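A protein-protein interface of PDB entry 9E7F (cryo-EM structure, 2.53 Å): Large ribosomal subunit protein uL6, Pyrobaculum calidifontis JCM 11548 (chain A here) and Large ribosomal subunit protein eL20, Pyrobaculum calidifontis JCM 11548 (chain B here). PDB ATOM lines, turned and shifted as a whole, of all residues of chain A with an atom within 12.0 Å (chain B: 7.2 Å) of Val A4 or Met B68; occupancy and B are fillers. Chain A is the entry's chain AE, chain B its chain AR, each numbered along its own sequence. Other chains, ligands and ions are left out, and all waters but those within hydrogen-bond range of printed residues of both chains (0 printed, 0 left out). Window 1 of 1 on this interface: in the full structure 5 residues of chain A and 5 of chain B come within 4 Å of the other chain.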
ATOM      1  N   MET A   1     -12.230 -10.986  -9.330  1.00  0.00           N
ATOM      2  CA  MET A   1     -12.198 -10.301 -10.614  1.00  0.00           C
ATOM      3  C   MET A   1     -11.757 -11.237 -11.733  1.00  0.00           C
ATOM      4  O   MET A   1     -10.873 -12.067 -11.550  1.00  0.00           O
ATOM      5  CB  MET A   1     -11.272  -9.083 -10.546  1.00  0.00           C
ATOM      6  CG  MET A   1     -10.863  -8.516 -11.901  1.00  0.00           C
ATOM      7  SD  MET A   1     -12.119  -7.502 -12.699  1.00  0.00           S
ATOM      8  CE  MET A   1     -13.130  -7.055 -11.296  1.00  0.00           C
ATOM      9  N   HIS A   2     -12.388 -11.083 -12.893  1.00  0.00           N
ATOM     10  CA  HIS A   2     -12.073 -11.839 -14.095  1.00  0.00           C
ATOM     11  C   HIS A   2     -10.679 -11.450 -14.564  1.00  0.00           C
ATOM     12  O   HIS A   2     -10.156 -10.407 -14.176  1.00  0.00           O
ATOM     13  CB  HIS A   2     -13.121 -11.568 -15.190  1.00  0.00           C
ATOM     14  CG  HIS A   2     -13.033 -12.492 -16.366  1.00  0.00           C
ATOM     15  ND1 HIS A   2     -13.193 -13.855 -16.249  1.00  0.00           N
ATOM     16  CD2 HIS A   2     -12.814 -12.250 -17.679  1.00  0.00           C
ATOM     17  CE1 HIS A   2     -13.064 -14.413 -17.438  1.00  0.00           C
ATOM     18  NE2 HIS A   2     -12.836 -13.462 -18.324  1.00  0.00           N
ATOM     19  N   VAL A   3     -10.042 -12.331 -15.332  1.00  0.00           N
ATOM     20  CA  VAL A   3      -8.789 -12.028 -16.019  1.00  0.00           C
ATOM     21  C   VAL A   3      -8.841 -12.656 -17.403  1.00  0.00           C
ATOM     22  O   VAL A   3      -9.321 -13.784 -17.564  1.00  0.00           O
ATOM     23  CB  VAL A   3      -7.556 -12.527 -15.232  1.00  0.00           C
ATOM     24  CG1 VAL A   3      -6.286 -12.305 -16.026  1.00  0.00           C
ATOM     25  CG2 VAL A   3      -7.451 -11.811 -13.904  1.00  0.00           C
ATOM     26  N   VAL A   4      -8.358 -11.923 -18.401  1.00  0.00           N
ATOM     27  CA  VAL A   4      -8.323 -12.429 -19.771  1.00  0.00           C
ATOM     28  C   VAL A   4      -6.995 -13.107 -20.078  1.00  0.00           C
ATOM     29  O   VAL A   4      -6.964 -14.231 -20.582  1.00  0.00           O
ATOM     30  CB  VAL A   4      -8.619 -11.290 -20.769  1.00  0.00           C
ATOM     31  CG1 VAL A   4      -8.376 -11.756 -22.190  1.00  0.00           C
ATOM     32  CG2 VAL A   4     -10.045 -10.805 -20.608  1.00  0.00           C
ATOM     33  N   TYR A   5      -5.880 -12.437 -19.788  1.00  0.00           N
ATOM     34  CA  TYR A   5      -4.561 -13.034 -19.947  1.00  0.00           C
ATOM     35  C   TYR A   5      -3.735 -12.621 -18.739  1.00  0.00           C
ATOM     36  O   TYR A   5      -3.755 -11.456 -18.340  1.00  0.00           O
ATOM     37  CB  TYR A   5      -3.900 -12.593 -21.273  1.00  0.00           C
ATOM     38  CG  TYR A   5      -2.624 -13.331 -21.716  1.00  0.00           C
ATOM     39  CD1 TYR A   5      -1.454 -13.334 -20.956  1.00  0.00           C
ATOM     40  CD2 TYR A   5      -2.608 -14.039 -22.903  1.00  0.00           C
ATOM     41  CE1 TYR A   5      -0.332 -14.008 -21.359  1.00  0.00           C
ATOM     42  CE2 TYR A   5      -1.478 -14.720 -23.319  1.00  0.00           C
ATOM     43  CZ  TYR A   5      -0.345 -14.699 -22.541  1.00  0.00           C
ATOM     44  OH  TYR A   5       0.787 -15.372 -22.941  1.00  0.00           O
ATOM     45  N   ALA A   6      -3.008 -13.581 -18.176  1.00  0.00           N
ATOM     46  CA  ALA A   6      -1.985 -13.319 -17.177  1.00  0.00           C
ATOM     47  C   ALA A   6      -0.755 -14.151 -17.504  1.00  0.00           C
ATOM     48  O   ALA A   6      -0.860 -15.247 -18.057  1.00  0.00           O
ATOM     49  CB  ALA A   6      -2.478 -13.632 -15.766  1.00  0.00           C
ATOM     50  N   VAL A   7       0.417 -13.619 -17.172  1.00  0.00           N
ATOM     51  CA  VAL A   7       1.682 -14.263 -17.506  1.00  0.00           C
ATOM     52  C   VAL A   7       2.656 -14.110 -16.350  1.00  0.00           C
ATOM     53  O   VAL A   7       2.731 -13.051 -15.718  1.00  0.00           O
ATOM     54  CB  VAL A   7       2.289 -13.689 -18.799  1.00  0.00           C
ATOM     55  CG1 VAL A   7       2.588 -12.211 -18.629  1.00  0.00           C
ATOM     56  CG2 VAL A   7       3.538 -14.454 -19.174  1.00  0.00           C
ATOM     57  N   GLU A   8       3.397 -15.180 -16.072  1.00  0.00           N
ATOM     58  CA  GLU A   8       4.504 -15.156 -15.130  1.00  0.00           C
ATOM     59  C   GLU A   8       5.654 -15.960 -15.711  1.00  0.00           C
ATOM     60  O   GLU A   8       5.465 -17.073 -16.202  1.00  0.00           O
ATOM     61  CB  GLU A   8       4.111 -15.728 -13.764  1.00  0.00           C
ATOM     62  CG  GLU A   8       3.173 -14.842 -12.971  1.00  0.00           C
ATOM     63  CD  GLU A   8       3.860 -14.140 -11.821  1.00  0.00           C
ATOM     64  OE1 GLU A   8       4.106 -14.792 -10.784  1.00  0.00           O
ATOM     65  OE2 GLU A   8       4.154 -12.935 -11.950  1.00  0.00           O
ATOM     66  N   PRO A  47      -5.265 -25.158 -14.572  1.00  0.00           N
ATOM     67  CA  PRO A  47      -5.529 -24.211 -15.656  1.00  0.00           C
ATOM     68  C   PRO A  47      -4.289 -23.472 -16.105  1.00  0.00           C
ATOM     69  O   PRO A  47      -4.284 -22.921 -17.213  1.00  0.00           O
ATOM     70  CB  PRO A  47      -6.545 -23.251 -15.036  1.00  0.00           C
ATOM     71  CG  PRO A  47      -6.210 -23.273 -13.590  1.00  0.00           C
ATOM     72  CD  PRO A  47      -5.736 -24.660 -13.272  1.00  0.00           C
ATOM     73  N   VAL A  48      -3.240 -23.452 -15.278  1.00  0.00           N
ATOM     74  CA  VAL A  48      -2.020 -22.736 -15.616  1.00  0.00           C
ATOM     75  C   VAL A  48      -1.324 -23.424 -16.777  1.00  0.00           C
ATOM     76  O   VAL A  48      -1.200 -24.654 -16.814  1.00  0.00           O
ATOM     77  CB  VAL A  48      -1.097 -22.657 -14.390  1.00  0.00           C
ATOM     78  CG1 VAL A  48       0.098 -21.774 -14.680  1.00  0.00           C
ATOM     79  CG2 VAL A  48      -1.862 -22.143 -13.191  1.00  0.00           C
ATOM     80  N   ILE A  49      -0.874 -22.632 -17.738  1.00  0.00           N
ATOM     81  CA  ILE A  49      -0.153 -23.148 -18.893  1.00  0.00           C
ATOM     82  C   ILE A  49       1.336 -23.088 -18.598  1.00  0.00           C
ATOM     83  O   ILE A  49       1.868 -22.024 -18.263  1.00  0.00           O
ATOM     84  CB  ILE A  49      -0.494 -22.351 -20.160  1.00  0.00           C
ATOM     85  CG1 ILE A  49      -1.979 -22.491 -20.498  1.00  0.00           C
ATOM     86  CG2 ILE A  49       0.368 -22.818 -21.318  1.00  0.00           C
ATOM     87  CD1 ILE A  49      -2.303 -23.706 -21.321  1.00  0.00           C
ATOM     88  N   LEU A  59       4.540 -19.251 -17.465  1.00  0.00           N
ATOM     89  CA  LEU A  59       3.260 -19.559 -16.844  1.00  0.00           C
ATOM     90  C   LEU A  59       2.239 -18.533 -17.303  1.00  0.00           C
ATOM     91  O   LEU A  59       2.452 -17.327 -17.140  1.00  0.00           O
ATOM     92  CB  LEU A  59       3.372 -19.565 -15.320  1.00  0.00           C
ATOM     93  CG  LEU A  59       4.567 -20.306 -14.725  1.00  0.00           C
ATOM     94  CD1 LEU A  59       4.701 -19.983 -13.250  1.00  0.00           C
ATOM     95  CD2 LEU A  59       4.416 -21.799 -14.938  1.00  0.00           C
ATOM     96  N   GLU A  60       1.134 -19.007 -17.872  1.00  0.00           N
ATOM     97  CA  GLU A  60       0.079 -18.126 -18.347  1.00  0.00           C
ATOM     98  C   GLU A  60      -1.277 -18.757 -18.085  1.00  0.00           C
ATOM     99  O   GLU A  60      -1.403 -19.977 -17.963  1.00  0.00           O
ATOM    100  CB  GLU A  60       0.215 -17.822 -19.841  1.00  0.00           C
ATOM    101  CG  GLU A  60       0.058 -19.031 -20.724  1.00  0.00           C
ATOM    102  CD  GLU A  60       1.383 -19.629 -21.129  1.00  0.00           C
ATOM    103  OE1 GLU A  60       2.095 -20.148 -20.247  1.00  0.00           O
ATOM    104  OE2 GLU A  60       1.712 -19.589 -22.331  1.00  0.00           O
ATOM    105  N   VAL A  61      -2.292 -17.903 -18.002  1.00  0.00           N
ATOM    106  CA  VAL A  61      -3.676 -18.329 -17.861  1.00  0.00           C
ATOM    107  C   VAL A  61      -4.509 -17.579 -18.886  1.00  0.00           C
ATOM    108  O   VAL A  61      -4.093 -16.543 -19.415  1.00  0.00           O
ATOM    109  CB  VAL A  61      -4.219 -18.086 -16.440  1.00  0.00           C
ATOM    110  CG1 VAL A  61      -3.855 -19.241 -15.531  1.00  0.00           C
ATOM    111  CG2 VAL A  61      -3.689 -16.782 -15.891  1.00  0.00           C
ATOM    112  N   LEU A  62      -5.686 -18.121 -19.182  1.00  0.00           N
ATOM    113  CA  LEU A  62      -6.617 -17.523 -20.126  1.00  0.00           C
ATOM    114  C   LEU A  62      -8.028 -17.724 -19.606  1.00  0.00           C
ATOM    115  O   LEU A  62      -8.408 -18.852 -19.280  1.00  0.00           O
ATOM    116  CB  LEU A  62      -6.474 -18.153 -21.511  1.00  0.00           C
ATOM    117  CG  LEU A  62      -5.090 -18.077 -22.148  1.00  0.00           C
ATOM    118  CD1 LEU A  62      -4.949 -19.155 -23.204  1.00  0.00           C
ATOM    119  CD2 LEU A  62      -4.847 -16.704 -22.744  1.00  0.00           C
ATOM    120  N   ASN A  63      -8.802 -16.637 -19.542  1.00  0.00           N
ATOM    121  CA  ASN A  63     -10.172 -16.680 -19.032  1.00  0.00           C
ATOM    122  C   ASN A  63     -10.179 -17.152 -17.580  1.00  0.00           C
ATOM    123  O   ASN A  63     -10.830 -18.135 -17.223  1.00  0.00           O
ATOM    124  CB  ASN A  63     -11.048 -17.579 -19.910  1.00  0.00           C
ATOM    125  CG  ASN A  63     -12.535 -17.361 -19.693  1.00  0.00           C
ATOM    126  OD1 ASN A  63     -13.020 -17.293 -18.565  1.00  0.00           O
ATOM    127  ND2 ASN A  63     -13.270 -17.258 -20.789  1.00  0.00           N
ATOM    128  N   ALA A  64      -9.433 -16.450 -16.739  1.00  0.00           N
ATOM    129  CA  ALA A  64      -9.166 -16.903 -15.388  1.00  0.00           C
ATOM    130  C   ALA A  64      -9.849 -16.004 -14.369  1.00  0.00           C
ATOM    131  O   ALA A  64      -9.874 -14.779 -14.510  1.00  0.00           O
ATOM    132  CB  ALA A  64      -7.662 -16.946 -15.114  1.00  0.00           C
ATOM    133  N   LYS A  65     -10.408 -16.631 -13.342  1.00  0.00           N
ATOM    134  CA  LYS A  65     -10.960 -15.914 -12.208  1.00  0.00           C
ATOM    135  C   LYS A  65      -9.858 -15.735 -11.169  1.00  0.00           C
ATOM    136  O   LYS A  65      -8.686 -16.024 -11.422  1.00  0.00           O
ATOM    137  CB  LYS A  65     -12.169 -16.654 -11.643  1.00  0.00           C
ATOM    138  CG  LYS A  65     -13.437 -16.504 -12.470  1.00  0.00           C
ATOM    139  CD  LYS A  65     -14.227 -15.259 -12.088  1.00  0.00           C
ATOM    140  CE  LYS A  65     -14.352 -14.304 -13.268  1.00  0.00           C
ATOM    141  NZ  LYS A  65     -15.593 -13.481 -13.224  1.00  0.00           N
ATOM    142  N   LYS A  66     -10.222 -15.255  -9.983  1.00  0.00           N
ATOM    143  CA  LYS A  66      -9.225 -15.042  -8.941  1.00  0.00           C
ATOM    144  C   LYS A  66      -8.663 -16.365  -8.442  1.00  0.00           C
ATOM    145  O   LYS A  66      -7.487 -16.454  -8.080  1.00  0.00           O
ATOM    146  CB  LYS A  66      -9.835 -14.243  -7.789  1.00  0.00           C
ATOM    147  CG  LYS A  66      -8.854 -13.312  -7.097  1.00  0.00           C
ATOM    148  CD  LYS A  66      -8.160 -12.385  -8.089  1.00  0.00           C
ATOM    149  CE  LYS A  66      -9.136 -11.763  -9.072  1.00  0.00           C
ATOM    150  NZ  LYS A  66      -8.440 -11.140 -10.224  1.00  0.00           N
ATOM    151  N   ARG A  67      -9.498 -17.404  -8.407  1.00  0.00           N
ATOM    152  CA  ARG A  67      -9.041 -18.710  -7.946  1.00  0.00           C
ATOM    153  C   ARG A  67      -7.974 -19.278  -8.870  1.00  0.00           C
ATOM    154  O   ARG A  67      -6.962 -19.815  -8.407  1.00  0.00           O
ATOM    155  CB  ARG A  67     -10.228 -19.664  -7.839  1.00  0.00           C
ATOM    156  CG  ARG A  67      -9.844 -21.125  -7.709  1.00  0.00           C
ATOM    157  CD  ARG A  67     -10.998 -22.040  -8.079  1.00  0.00           C
ATOM    158  NE  ARG A  67     -12.289 -21.461  -7.733  1.00  0.00           N
ATOM    159  CZ  ARG A  67     -13.203 -21.087  -8.618  1.00  0.00           C
ATOM    160  NH1 ARG A  67     -13.001 -21.219  -9.918  1.00  0.00           N
ATOM    161  NH2 ARG A  67     -14.350 -20.569  -8.186  1.00  0.00           N
ATOM    162  N   GLU A  68      -8.176 -19.159 -10.180  1.00  0.00           N
ATOM    163  CA  GLU A  68      -7.193 -19.650 -11.136  1.00  0.00           C
ATOM    164  C   GLU A  68      -6.006 -18.705 -11.252  1.00  0.00           C
ATOM    165  O   GLU A  68      -4.876 -19.149 -11.476  1.00  0.00           O
ATOM    166  CB  GLU A  68      -7.849 -19.844 -12.499  1.00  0.00           C
ATOM    167  CG  GLU A  68      -8.590 -21.156 -12.637  1.00  0.00           C
ATOM    168  CD  GLU A  68      -9.892 -21.020 -13.398  1.00  0.00           C
ATOM    169  OE1 GLU A  68     -10.803 -20.328 -12.901  1.00  0.00           O
ATOM    170  OE2 GLU A  68     -10.004 -21.605 -14.495  1.00  0.00           O
ATOM    171  N   TYR A  69      -6.244 -17.404 -11.104  1.00  0.00           N
ATOM    172  CA  TYR A  69      -5.191 -16.425 -11.349  1.00  0.00           C
ATOM    173  C   TYR A  69      -4.106 -16.493 -10.281  1.00  0.00           C
ATOM    174  O   TYR A  69      -2.920 -16.336 -10.584  1.00  0.00           O
ATOM    175  CB  TYR A  69      -5.792 -15.024 -11.421  1.00  0.00           C
ATOM    176  CG  TYR A  69      -4.791 -13.930 -11.187  1.00  0.00           C
ATOM    177  CD1 TYR A  69      -3.813 -13.650 -12.125  1.00  0.00           C
ATOM    178  CD2 TYR A  69      -4.814 -13.186 -10.021  1.00  0.00           C
ATOM    179  CE1 TYR A  69      -2.891 -12.658 -11.914  1.00  0.00           C
ATOM    180  CE2 TYR A  69      -3.894 -12.191  -9.800  1.00  0.00           C
ATOM    181  CZ  TYR A  69      -2.936 -11.932 -10.750  1.00  0.00           C
ATOM    182  OH  TYR A  69      -2.020 -10.937 -10.530  1.00  0.00           O
ATOM    183  N   ALA A  70      -4.486 -16.748  -9.030  1.00  0.00           N
ATOM    184  CA  ALA A  70      -3.509 -16.837  -7.953  1.00  0.00           C
ATOM    185  C   ALA A  70      -2.596 -18.049  -8.069  1.00  0.00           C
ATOM    186  O   ALA A  70      -1.578 -18.102  -7.373  1.00  0.00           O
ATOM    187  CB  ALA A  70      -4.221 -16.860  -6.603  1.00  0.00           C
ATOM    188  N   LEU A  72      -0.858 -18.724 -10.683  1.00  0.00           N
ATOM    189  CA  LEU A  72       0.372 -18.310 -11.351  1.00  0.00           C
ATOM    190  C   LEU A  72       1.457 -17.988 -10.337  1.00  0.00           C
ATOM    191  O   LEU A  72       2.578 -18.499 -10.427  1.00  0.00           O
ATOM    192  CB  LEU A  72       0.117 -17.098 -12.245  1.00  0.00           C
ATOM    193  CG  LEU A  72      -0.674 -17.281 -13.533  1.00  0.00           C
ATOM    194  CD1 LEU A  72      -0.635 -15.996 -14.322  1.00  0.00           C
ATOM    195  CD2 LEU A  72      -0.094 -18.414 -14.339  1.00  0.00           C
ATOM    196  N   ILE B   4     -15.355  -0.759 -27.637  1.00  0.00           N
ATOM    197  CA  ILE B   4     -15.666  -0.597 -26.224  1.00  0.00           C
ATOM    198  C   ILE B   4     -16.793   0.414 -26.110  1.00  0.00           C
ATOM    199  O   ILE B   4     -16.656   1.558 -26.559  1.00  0.00           O
ATOM    200  CB  ILE B   4     -14.433  -0.144 -25.427  1.00  0.00           C
ATOM    201  CG1 ILE B   4     -13.286  -1.129 -25.621  1.00  0.00           C
ATOM    202  CG2 ILE B   4     -14.756  -0.054 -23.953  1.00  0.00           C
ATOM    203  CD1 ILE B   4     -11.948  -0.577 -25.224  1.00  0.00           C
ATOM    204  N   VAL B  22     -17.141  -4.657 -24.554  1.00  0.00           N
ATOM    205  CA  VAL B  22     -16.579  -4.815 -25.887  1.00  0.00           C
ATOM    206  C   VAL B  22     -17.579  -5.611 -26.713  1.00  0.00           C
ATOM    207  O   VAL B  22     -17.750  -6.814 -26.504  1.00  0.00           O
ATOM    208  CB  VAL B  22     -15.210  -5.503 -25.845  1.00  0.00           C
ATOM    209  CG1 VAL B  22     -14.628  -5.610 -27.240  1.00  0.00           C
ATOM    210  CG2 VAL B  22     -14.274  -4.738 -24.930  1.00  0.00           C
ATOM    211  N   SER B  63     -11.479   0.106 -18.094  1.00  0.00           N
ATOM    212  CA  SER B  63     -11.425  -1.333 -17.896  1.00  0.00           C
ATOM    213  C   SER B  63     -10.244  -1.909 -18.659  1.00  0.00           C
ATOM    214  O   SER B  63     -10.160  -1.762 -19.880  1.00  0.00           O
ATOM    215  CB  SER B  63     -12.716  -2.001 -18.362  1.00  0.00           C
ATOM    216  OG  SER B  63     -12.449  -3.315 -18.814  1.00  0.00           O
ATOM    217  N   ASN B  64      -9.330  -2.561 -17.939  1.00  0.00           N
ATOM    218  CA  ASN B  64      -8.261  -3.291 -18.607  1.00  0.00           C
ATOM    219  C   ASN B  64      -8.799  -4.510 -19.343  1.00  0.00           C
ATOM    220  O   ASN B  64      -8.200  -4.953 -20.330  1.00  0.00           O
ATOM    221  CB  ASN B  64      -7.196  -3.707 -17.598  1.00  0.00           C
ATOM    222  CG  ASN B  64      -7.054  -2.720 -16.467  1.00  0.00           C
ATOM    223  OD1 ASN B  64      -7.791  -2.777 -15.482  1.00  0.00           O
ATOM    224  ND2 ASN B  64      -6.095  -1.809 -16.594  1.00  0.00           N
ATOM    225  N   GLU B  65      -9.916  -5.064 -18.878  1.00  0.00           N
ATOM    226  CA  GLU B  65     -10.498  -6.224 -19.537  1.00  0.00           C
ATOM    227  C   GLU B  65     -11.015  -5.845 -20.920  1.00  0.00           C
ATOM    228  O   GLU B  65     -10.942  -6.643 -21.860  1.00  0.00           O
ATOM    229  CB  GLU B  65     -11.621  -6.786 -18.663  1.00  0.00           C
ATOM    230  CG  GLU B  65     -11.263  -6.914 -17.162  1.00  0.00           C
ATOM    231  CD  GLU B  65     -10.052  -7.794 -16.816  1.00  0.00           C
ATOM    232  OE1 GLU B  65      -9.973  -8.201 -15.644  1.00  0.00           O
ATOM    233  OE2 GLU B  65      -9.193  -8.096 -17.667  1.00  0.00           O
ATOM    234  N   ALA B  66     -11.536  -4.624 -21.053  1.00  0.00           N
ATOM    235  CA  ALA B  66     -11.918  -4.107 -22.361  1.00  0.00           C
ATOM    236  C   ALA B  66     -10.710  -3.974 -23.277  1.00  0.00           C
ATOM    237  O   ALA B  66     -10.763  -4.366 -24.448  1.00  0.00           O
ATOM    238  CB  ALA B  66     -12.610  -2.755 -22.200  1.00  0.00           C
ATOM    239  N   LYS B  67      -9.613  -3.418 -22.762  1.00  0.00           N
ATOM    240  CA  LYS B  67      -8.425  -3.230 -23.588  1.00  0.00           C
ATOM    241  C   LYS B  67      -7.794  -4.562 -23.963  1.00  0.00           C
ATOM    242  O   LYS B  67      -7.275  -4.716 -25.074  1.00  0.00           O
ATOM    243  CB  LYS B  67      -7.415  -2.341 -22.868  1.00  0.00           C
ATOM    244  CG  LYS B  67      -8.029  -1.333 -21.929  1.00  0.00           C
ATOM    245  CD  LYS B  67      -7.225  -0.045 -21.913  1.00  0.00           C
ATOM    246  CE  LYS B  67      -5.885  -0.213 -21.218  1.00  0.00           C
ATOM    247  NZ  LYS B  67      -5.969   0.001 -19.753  1.00  0.00           N
ATOM    248  N   MET B  68      -7.816  -5.533 -23.053  1.00  0.00           N
ATOM    249  CA  MET B  68      -7.248  -6.836 -23.370  1.00  0.00           C
ATOM    250  C   MET B  68      -8.106  -7.588 -24.381  1.00  0.00           C
ATOM    251  O   MET B  68      -7.575  -8.268 -25.267  1.00  0.00           O
ATOM    252  CB  MET B  68      -7.072  -7.653 -22.095  1.00  0.00           C
ATOM    253  CG  MET B  68      -5.749  -7.417 -21.401  1.00  0.00           C
ATOM    254  SD  MET B  68      -5.304  -8.776 -20.309  1.00  0.00           S
ATOM    255  CE  MET B  68      -6.581  -8.642 -19.066  1.00  0.00           C
ATOM    256  N   LEU B  69      -9.431  -7.489 -24.264  1.00  0.00           N
ATOM    257  CA  LEU B  69     -10.298  -8.222 -25.180  1.00  0.00           C
ATOM    258  C   LEU B  69     -10.245  -7.656 -26.590  1.00  0.00           C
ATOM    259  O   LEU B  69     -10.492  -8.388 -27.555  1.00  0.00           O
ATOM    260  CB  LEU B  69     -11.739  -8.218 -24.674  1.00  0.00           C
ATOM    261  CG  LEU B  69     -12.030  -9.002 -23.401  1.00  0.00           C
ATOM    262  CD1 LEU B  69     -13.453  -8.754 -22.966  1.00  0.00           C
ATOM    263  CD2 LEU B  69     -11.795 -10.476 -23.629  1.00  0.00           C
ATOM    264  N   MET B  70      -9.942  -6.367 -26.733  1.00  0.00           N
ATOM    265  CA  MET B  70      -9.916  -5.764 -28.060  1.00  0.00           C
ATOM    266  C   MET B  70      -8.779  -6.326 -28.904  1.00  0.00           C
ATOM    267  O   MET B  70      -8.936  -6.537 -30.110  1.00  0.00           O
ATOM    268  CB  MET B  70      -9.801  -4.248 -27.948  1.00  0.00           C
ATOM    269  CG  MET B  70     -11.090  -3.563 -27.543  1.00  0.00           C
ATOM    270  SD  MET B  70     -11.980  -2.882 -28.954  1.00  0.00           S
ATOM    271  CE  MET B  70     -10.666  -2.011 -29.800  1.00  0.00           C
ATOM    272  N   VAL B  71      -7.626  -6.580 -28.286  1.00  0.00           N
ATOM    273  CA  VAL B  71      -6.456  -7.071 -29.003  1.00  0.00           C
ATOM    274  C   VAL B  71      -6.328  -8.590 -28.921  1.00  0.00           C
ATOM    275  O   VAL B  71      -5.279  -9.137 -29.271  1.00  0.00           O
ATOM    276  CB  VAL B  71      -5.177  -6.384 -28.501  1.00  0.00           C
ATOM    277  CG1 VAL B  71      -5.300  -4.888 -28.655  1.00  0.00           C
ATOM    278  CG2 VAL B  71      -4.914  -6.744 -27.059  1.00  0.00           C
ATOM    279  N   LEU B  72      -7.368  -9.278 -28.465  1.00  0.00           N
ATOM    280  CA  LEU B  72      -7.330 -10.730 -28.378  1.00  0.00           C
ATOM    281  C   LEU B  72      -7.214 -11.341 -29.766  1.00  0.00           C
ATOM    282  O   LEU B  72      -7.978 -11.006 -30.673  1.00  0.00           O
ATOM    283  CB  LEU B  72      -8.585 -11.244 -27.677  1.00  0.00           C
ATOM    284  CG  LEU B  72      -8.414 -12.463 -26.777  1.00  0.00           C
ATOM    285  CD1 LEU B  72      -7.574 -12.131 -25.568  1.00  0.00           C
ATOM    286  CD2 LEU B  72      -9.777 -12.987 -26.366  1.00  0.00           C
ATOM    287  N   GLU B  73      -6.249 -12.240 -29.930  1.00  0.00           N
ATOM    288  CA  GLU B  73      -5.942 -12.802 -31.232  1.00  0.00           C
ATOM    289  C   GLU B  73      -6.410 -14.235 -31.397  1.00  0.00           C
ATOM    290  O   GLU B  73      -6.373 -14.751 -32.518  1.00  0.00           O
ATOM    291  CB  GLU B  73      -4.430 -12.729 -31.493  1.00  0.00           C
ATOM    292  CG  GLU B  73      -3.844 -11.340 -31.271  1.00  0.00           C
ATOM    293  CD  GLU B  73      -4.010 -10.434 -32.472  1.00  0.00           C
ATOM    294  OE1 GLU B  73      -3.793 -10.900 -33.609  1.00  0.00           O
ATOM    295  OE2 GLU B  73      -4.374  -9.258 -32.279  1.00  0.00           O
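Among the printed residues, merely in contact across the chains: Val A4 with Leu B72 (3.5 Å), Val A4 with Leu B69 (3.5 Å), Val A4 with Met B68 (3.8 Å) and Val A4 with Glu B65 (3.99 Å).
Of the printed residues of chain B, Met A1 touches Glu B65 (3.7 Å). Of the printed residues of chain B, His A2 touches Glu B65. Printed residues of chain B within 4 Å of Val A4: Glu B65 (3.99 Å), Met B68 (3.8 Å), Leu B69 (3.5 Å) and Leu B72 (3.5 Å). Of the printed residues of chain B, Tyr A5 touches Met B68 (3.7 Å). Leu A62 touches none of the printed residues of chain B. Glu A68 touches none of the printed residues of chain B. No residue of chain A comes within 4 Å of Asn B64. Printed residues of chain A within 4 Å of Glu B65: Met A1 (3.7 Å), His A2 (2.7 Å) and Val A4 (3.99 Å). No residue of chain A comes within 4 Å of Ala B66. No residue of chain A comes within 4 Å of Lys B67. Met B68 touches two residues of chain A. Of chain A, only Val A4 (3.5 Å) comes within 4 Å of Leu B69. No residue of chain A comes within 4 Å of Val B71. The nearest printed residue of chain B that does not touch Val A4 is Asn B64 (6.1 Å). The nearest residue of chain A that does not touch Met B68 is Val A3 (4.8 Å). The nearest printed residue of chain A that does not touch Glu B65 is Val A3 (4.02 Å).
The backbone carbonyl oxygen (O) of Met A1 lies within hydrogen-bond range of the side-chain amino group (NZ) of Lys A66 (2.9 Å). OG of Ser B63 lies within hydrogen-bond range of N of Glu B65. The backbone NH (N) of Asn A63 is in hydrogen-bond range of the backbone carbonyl oxygen (O) of Val A4 (3.2 Å).
Of the 13 printed residues of chain B, 4 touch a printed residue of chain A. Hydrophobic or aromatic side chains of chain B that line the printed part of chain A: Met B68, Leu B69 and Leu B72. Of the 24 printed residues of chain A, 4 touch a printed residue of chain B. Among the printed residues, 7 pairs touch across the chains.
SD of Met B68 lies within hydrogen-bond range of N of Tyr A5, at 3.7 Å. The backbone carbonyl oxygen of His A2 sits close to the side-chain carboxylate of Glu B65. SD of Met A1 lies close to OE1 of Glu B65.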
